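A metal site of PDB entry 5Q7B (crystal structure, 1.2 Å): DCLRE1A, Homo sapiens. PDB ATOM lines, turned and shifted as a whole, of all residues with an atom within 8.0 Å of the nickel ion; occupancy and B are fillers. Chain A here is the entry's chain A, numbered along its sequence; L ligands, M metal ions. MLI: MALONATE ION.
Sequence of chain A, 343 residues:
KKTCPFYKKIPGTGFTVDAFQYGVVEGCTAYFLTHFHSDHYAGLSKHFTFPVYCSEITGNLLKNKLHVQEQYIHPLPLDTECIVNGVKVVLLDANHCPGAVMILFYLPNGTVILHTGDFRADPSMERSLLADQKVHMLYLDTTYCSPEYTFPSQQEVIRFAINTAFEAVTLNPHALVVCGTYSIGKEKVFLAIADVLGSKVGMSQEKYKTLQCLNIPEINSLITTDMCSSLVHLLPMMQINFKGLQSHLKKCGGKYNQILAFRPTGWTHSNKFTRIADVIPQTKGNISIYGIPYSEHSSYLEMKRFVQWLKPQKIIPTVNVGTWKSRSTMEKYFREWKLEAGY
A ring nitrogen (NE2) of His 40 sits close to the side-chain carboxylate of Asp 118.
O of Ile 184 sits at hydrogen-bond distance from NE2 of His 37 (2.9 Å).
ND1 of His 35 lies within hydrogen-bond range of OG1 of Thr 34 (2.9 Å).
ND1 of His 96 sits at hydrogen-bond distance from O of Glu 296 (2.8 Å).
Of the 20 residues printed, 4 come within 4 Å of the nickel ion.
The nearest printed residue that does not touch the nickel ion is His 40 (4.3 Å).
O8 of the ligand binds the nickel ion (2.1 Å).
The nickel ion is bound by an oxygen (O7) of the ligand, 2.1 Å away.
OD2 of Asp 118 binds the nickel ion (2.2 Å).
A ring nitrogen (ND1) of His 37 binds the nickel ion, at 2.2 Å.
NE2 of His 35 is bound to the nickel ion, at 2.2 Å.
The nickel ion is bound by a ring nitrogen (NE2) of His 96 (2.2 Å).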
ATOM      1  N   ASP A  18      -2.145 -16.796  -5.929  1.00  0.00           N
ATOM      2  CA  ASP A  18      -1.288 -17.645  -5.029  1.00  0.00           C
ATOM      3  C   ASP A  18      -1.739 -19.162  -5.037  1.00  0.00           C
ATOM      4  O   ASP A  18      -1.810 -19.836  -3.976  1.00  0.00           O
ATOM      5  CB  ASP A  18      -1.132 -17.091  -3.656  1.00  0.00           C
ATOM      6  CG  ASP A  18      -0.515 -15.662  -3.618  1.00  0.00           C
ATOM      7  OD1 ASP A  18      -0.003 -15.227  -4.655  1.00  0.00           O
ATOM      8  OD2 ASP A  18      -0.661 -15.062  -2.517  1.00  0.00           O
ATOM      9  N   THR A  34       1.328 -12.819  -5.367  1.00  0.00           N
ATOM     10  CA  THR A  34       1.432 -11.600  -4.580  1.00  0.00           C
ATOM     11  C   THR A  34       2.874 -11.297  -4.079  1.00  0.00           C
ATOM     12  O   THR A  34       3.267 -10.135  -3.966  1.00  0.00           O
ATOM     13  CB  THR A  34       0.472 -11.640  -3.384  1.00  0.00           C
ATOM     14  OG1 THR A  34       0.826 -12.697  -2.423  1.00  0.00           O
ATOM     15  CG2 THR A  34      -0.972 -11.713  -3.796  1.00  0.00           C
ATOM     16  N   HIS A  35       3.643 -12.375  -3.766  1.00  0.00           N
ATOM     17  CA  HIS A  35       4.994 -12.256  -3.187  1.00  0.00           C
ATOM     18  C   HIS A  35       5.730 -13.558  -3.247  1.00  0.00           C
ATOM     19  O   HIS A  35       5.090 -14.643  -3.245  1.00  0.00           O
ATOM     20  CB  HIS A  35       4.947 -11.569  -1.780  1.00  0.00           C
ATOM     21  CG  HIS A  35       4.344 -12.394  -0.683  1.00  0.00           C
ATOM     22  ND1 HIS A  35       3.025 -12.780  -0.565  1.00  0.00           N
ATOM     23  CD2 HIS A  35       4.952 -12.916   0.417  1.00  0.00           C
ATOM     24  CE1 HIS A  35       2.873 -13.465   0.581  1.00  0.00           C
ATOM     25  NE2 HIS A  35       4.023 -13.511   1.186  1.00  0.00           N
ATOM     26  N   PHE A  36       7.052 -13.435  -3.121  1.00  0.00           N
ATOM     27  CA  PHE A  36       7.972 -14.628  -3.118  1.00  0.00           C
ATOM     28  C   PHE A  36       8.180 -15.258  -1.749  1.00  0.00           C
ATOM     29  O   PHE A  36       9.362 -15.178  -1.227  1.00  0.00           O
ATOM     30  CB  PHE A  36       9.316 -14.217  -3.784  1.00  0.00           C
ATOM     31  CG  PHE A  36      10.158 -15.409  -4.216  1.00  0.00           C
ATOM     32  CD1 PHE A  36       9.803 -16.104  -5.368  1.00  0.00           C
ATOM     33  CD2 PHE A  36      11.315 -15.766  -3.528  1.00  0.00           C
ATOM     34  CE1 PHE A  36      10.609 -17.185  -5.816  1.00  0.00           C
ATOM     35  CE2 PHE A  36      12.126 -16.846  -3.968  1.00  0.00           C
ATOM     36  CZ  PHE A  36      11.765 -17.542  -5.068  1.00  0.00           C
ATOM     37  N   HIS A  37       7.115 -15.808  -1.127  1.00  0.00           N
ATOM     38  CA  HIS A  37       7.206 -16.642   0.080  1.00  0.00           C
ATOM     39  C   HIS A  37       6.699 -18.046  -0.298  1.00  0.00           C
ATOM     40  O   HIS A  37       5.732 -18.189  -1.036  1.00  0.00           O
ATOM     41  CB  HIS A  37       6.443 -16.100   1.304  1.00  0.00           C
ATOM     42  CG  HIS A  37       7.165 -15.001   2.062  1.00  0.00           C
ATOM     43  ND1 HIS A  37       6.554 -14.167   2.979  1.00  0.00           N
ATOM     44  CD2 HIS A  37       8.474 -14.655   2.061  1.00  0.00           C
ATOM     45  CE1 HIS A  37       7.459 -13.370   3.537  1.00  0.00           C
ATOM     46  NE2 HIS A  37       8.614 -13.641   2.970  1.00  0.00           N
ATOM     47  N   SER A  38       7.364 -19.089   0.227  1.00  0.00           N
ATOM     48  CA  SER A  38       7.148 -20.466  -0.283  1.00  0.00           C
ATOM     49  C   SER A  38       5.745 -20.963  -0.076  1.00  0.00           C
ATOM     50  O   SER A  38       5.280 -21.693  -0.945  1.00  0.00           O
ATOM     51  CB  SER A  38       8.204 -21.462   0.258  1.00  0.00           C
ATOM     52  OG  SER A  38       8.182 -21.520   1.666  1.00  0.00           O
ATOM     53  N   ASP A  39       5.030 -20.587   0.976  1.00  0.00           N
ATOM     54  CA  ASP A  39       3.629 -21.091   1.148  1.00  0.00           C
ATOM     55  C   ASP A  39       2.773 -20.573  -0.015  1.00  0.00           C
ATOM     56  O   ASP A  39       1.742 -21.176  -0.324  1.00  0.00           O
ATOM     57  CB  ASP A  39       3.010 -20.709   2.446  1.00  0.00           C
ATOM     58  CG  ASP A  39       3.428 -21.626   3.656  1.00  0.00           C
ATOM     59  OD1 ASP A  39       4.194 -22.584   3.426  1.00  0.00           O
ATOM     60  OD2 ASP A  39       2.977 -21.291   4.753  1.00  0.00           O
ATOM     61  N   HIS A  40       3.150 -19.424  -0.630  1.00  0.00           N
ATOM     62  CA  HIS A  40       2.391 -18.775  -1.704  1.00  0.00           C
ATOM     63  C   HIS A  40       2.816 -19.166  -3.072  1.00  0.00           C
ATOM     64  O   HIS A  40       1.912 -19.326  -3.998  1.00  0.00           O
ATOM     65  CB  HIS A  40       2.458 -17.219  -1.504  1.00  0.00           C
ATOM     66  CG  HIS A  40       1.833 -16.781  -0.233  1.00  0.00           C
ATOM     67  ND1 HIS A  40       0.588 -16.189  -0.135  1.00  0.00           N
ATOM     68  CD2 HIS A  40       2.301 -16.847   1.034  1.00  0.00           C
ATOM     69  CE1 HIS A  40       0.288 -16.009   1.127  1.00  0.00           C
ATOM     70  NE2 HIS A  40       1.325 -16.391   1.857  1.00  0.00           N
ATOM     71  N   HIS A  96       4.970  -5.590   3.162  1.00  0.00           N
ATOM     72  CA  HIS A  96       5.320  -6.942   3.659  1.00  0.00           C
ATOM     73  C   HIS A  96       6.792  -7.126   3.371  1.00  0.00           C
ATOM     74  O   HIS A  96       7.603  -6.389   4.006  1.00  0.00           O
ATOM     75  CB  HIS A  96       4.341  -7.982   3.024  1.00  0.00           C
ATOM     76  CG  HIS A  96       4.466  -9.423   3.504  1.00  0.00           C
ATOM     77  ND1 HIS A  96       4.481  -9.794   4.825  1.00  0.00           N
ATOM     78  CD2 HIS A  96       4.671 -10.567   2.803  1.00  0.00           C
ATOM     79  CE1 HIS A  96       4.622 -11.121   4.916  1.00  0.00           C
ATOM     80  NE2 HIS A  96       4.737 -11.643   3.717  1.00  0.00           N
ATOM     81  N   CYS A  97       7.205  -8.048   2.562  1.00  0.00           N
ATOM     82  CA  CYS A  97       8.604  -8.251   2.132  1.00  0.00           C
ATOM     83  C   CYS A  97       8.883  -7.560   0.779  1.00  0.00           C
ATOM     84  O   CYS A  97       7.916  -7.098   0.126  1.00  0.00           O
ATOM     85  CB  CYS A  97       8.878  -9.742   2.035  1.00  0.00           C
ATOM     86  SG  CYS A  97       7.930 -10.637   0.728  1.00  0.00           S
ATOM     87  N   ALA A 100       6.347  -7.501  -2.518  1.00  0.00           N
ATOM     88  CA  ALA A 100       4.991  -7.917  -2.114  1.00  0.00           C
ATOM     89  C   ALA A 100       3.953  -6.873  -2.496  1.00  0.00           C
ATOM     90  O   ALA A 100       4.157  -5.672  -2.238  1.00  0.00           O
ATOM     91  CB  ALA A 100       4.919  -8.247  -0.652  1.00  0.00           C
ATOM     92  N   GLY A 117      -3.035  -9.923  -0.366  1.00  0.00           N
ATOM     93  CA  GLY A 117      -1.911 -10.794  -0.188  1.00  0.00           C
ATOM     94  C   GLY A 117      -1.578 -10.907   1.283  1.00  0.00           C
ATOM     95  O   GLY A 117      -2.440 -10.850   2.137  1.00  0.00           O
ATOM     96  N   ASP A 118      -0.295 -11.023   1.594  1.00  0.00           N
ATOM     97  CA  ASP A 118       0.233 -10.759   2.968  1.00  0.00           C
ATOM     98  C   ASP A 118       0.566  -9.244   3.095  1.00  0.00           C
ATOM     99  O   ASP A 118       1.180  -8.677   2.156  1.00  0.00           O
ATOM    100  CB  ASP A 118       1.480 -11.587   3.266  1.00  0.00           C
ATOM    101  CG  ASP A 118       1.216 -13.050   3.584  1.00  0.00           C
ATOM    102  OD1 ASP A 118       0.073 -13.470   3.812  1.00  0.00           O
ATOM    103  OD2 ASP A 118       2.192 -13.791   3.751  1.00  0.00           O
ATOM    104  N   PHE A 119       0.164  -8.611   4.171  1.00  0.00           N
ATOM    105  CA  PHE A 119       0.378  -7.143   4.329  1.00  0.00           C
ATOM    106  C   PHE A 119       0.581  -6.792   5.782  1.00  0.00           C
ATOM    107  O   PHE A 119       0.093  -7.452   6.705  1.00  0.00           O
ATOM    108  CB  PHE A 119      -0.698  -6.301   3.597  1.00  0.00           C
ATOM    109  CG  PHE A 119      -2.017  -5.960   4.325  1.00  0.00           C
ATOM    110  CD1 PHE A 119      -2.606  -4.724   4.235  1.00  0.00           C
ATOM    111  CD2 PHE A 119      -2.723  -6.941   5.069  1.00  0.00           C
ATOM    112  CE1 PHE A 119      -3.834  -4.449   4.798  1.00  0.00           C
ATOM    113  CE2 PHE A 119      -3.919  -6.588   5.744  1.00  0.00           C
ATOM    114  CZ  PHE A 119      -4.468  -5.356   5.583  1.00  0.00           C
ATOM    115  N   ASP A 141      -5.609 -10.668   4.719  1.00  0.00           N
ATOM    116  CA  ASP A 141      -4.543 -11.363   5.531  1.00  0.00           C
ATOM    117  C   ASP A 141      -4.886 -11.156   6.992  1.00  0.00           C
ATOM    118  O   ASP A 141      -4.690 -10.106   7.604  1.00  0.00           O
ATOM    119  CB  ASP A 141      -3.163 -10.755   5.252  1.00  0.00           C
ATOM    120  CG  ASP A 141      -2.075 -11.183   6.204  1.00  0.00           C
ATOM    121  OD1 ASP A 141      -2.325 -12.162   6.967  1.00  0.00           O
ATOM    122  OD2 ASP A 141      -1.005 -10.516   6.199  1.00  0.00           O
ATOM    123  N   THR A 143      -3.661 -13.036   9.593  1.00  0.00           N
ATOM    124  CA  THR A 143      -2.673 -13.764  10.422  1.00  0.00           C
ATOM    125  C   THR A 143      -2.818 -13.446  11.890  1.00  0.00           C
ATOM    126  O   THR A 143      -2.906 -14.433  12.732  1.00  0.00           O
ATOM    127  CB  THR A 143      -1.211 -13.440   9.885  1.00  0.00           C
ATOM    128  OG1 THR A 143      -1.021 -13.886   8.571  1.00  0.00           O
ATOM    129  CG2 THR A 143      -0.196 -14.055  10.787  1.00  0.00           C
ATOM    130  N   SER A 183      13.962 -16.683   4.577  1.00  0.00           N
ATOM    131  CA  SER A 183      13.095 -16.260   3.505  1.00  0.00           C
ATOM    132  C   SER A 183      13.515 -14.800   3.234  1.00  0.00           C
ATOM    133  O   SER A 183      14.325 -14.199   4.029  1.00  0.00           O
ATOM    134  CB  SER A 183      11.606 -16.277   3.924  1.00  0.00           C
ATOM    135  OG  SER A 183      11.359 -15.392   4.990  1.00  0.00           O
ATOM    136  N   ILE A 184      13.033 -14.196   2.187  1.00  0.00           N
ATOM    137  CA  ILE A 184      13.132 -12.751   2.053  1.00  0.00           C
ATOM    138  C   ILE A 184      12.229 -12.027   3.043  1.00  0.00           C
ATOM    139  O   ILE A 184      11.291 -12.635   3.619  1.00  0.00           O
ATOM    140  CB  ILE A 184      12.856 -12.223   0.598  1.00  0.00           C
ATOM    141  CG1 ILE A 184      11.460 -12.493   0.125  1.00  0.00           C
ATOM    142  CG2 ILE A 184      13.840 -12.839  -0.385  1.00  0.00           C
ATOM    143  CD1 ILE A 184      11.052 -11.714  -1.108  1.00  0.00           C
ATOM    144  N   GLU A 296       6.224  -8.375   9.804  1.00  0.00           N
ATOM    145  CA  GLU A 296       5.767  -7.923   8.480  1.00  0.00           C
ATOM    146  C   GLU A 296       4.255  -8.239   8.165  1.00  0.00           C
ATOM    147  O   GLU A 296       3.811  -8.213   7.030  1.00  0.00           O
ATOM    148  CB  GLU A 296       6.721  -8.365   7.375  1.00  0.00           C
ATOM    149  CG  GLU A 296       8.113  -7.639   7.426  1.00  0.00           C
ATOM    150  CD  GLU A 296       9.071  -7.903   6.295  1.00  0.00           C
ATOM    151  OE1 GLU A 296       8.956  -8.943   5.597  1.00  0.00           O
ATOM    152  OE2 GLU A 296      10.039  -7.067   6.164  1.00  0.00           O
ATOM    153  N   HIS A 297       3.541  -8.538   9.258  1.00  0.00           N
ATOM    154  CA  HIS A 297       2.060  -8.620   9.188  1.00  0.00           C
ATOM    155  C   HIS A 297       1.395  -7.595  10.135  1.00  0.00           C
ATOM    156  O   HIS A 297       1.974  -7.208  11.180  1.00  0.00           O
ATOM    157  CB  HIS A 297       1.570 -10.052   9.591  1.00  0.00           C
ATOM    158  CG  HIS A 297       1.976 -11.145   8.679  1.00  0.00           C
ATOM    159  ND1 HIS A 297       1.267 -11.533   7.572  1.00  0.00           N
ATOM    160  CD2 HIS A 297       3.006 -12.062   8.790  1.00  0.00           C
ATOM    161  CE1 HIS A 297       1.851 -12.580   6.994  1.00  0.00           C
ATOM    162  NE2 HIS A 297       2.915 -12.886   7.709  1.00  0.00           N
HETATM  163  C1  MLI L   1       5.147 -16.294   5.509  1.00  0.00           C
HETATM  164  C2  MLI L   1       4.825 -15.007   6.226  1.00  0.00           C
HETATM  165  C3  MLI L   1       4.265 -16.703   4.332  1.00  0.00           C
HETATM  166  O6  MLI L   1       4.784 -14.915   7.437  1.00  0.00           O
HETATM  167  O7  MLI L   1       4.687 -14.067   5.491  1.00  0.00           O
HETATM  168  O8  MLI L   1       4.032 -15.900   3.414  1.00  0.00           O
HETATM  169  O9  MLI L   1       3.891 -17.906   4.224  1.00  0.00           O
HETATM  170 NI    NI M   1       4.376 -13.834   3.379  1.00  0.00          NI
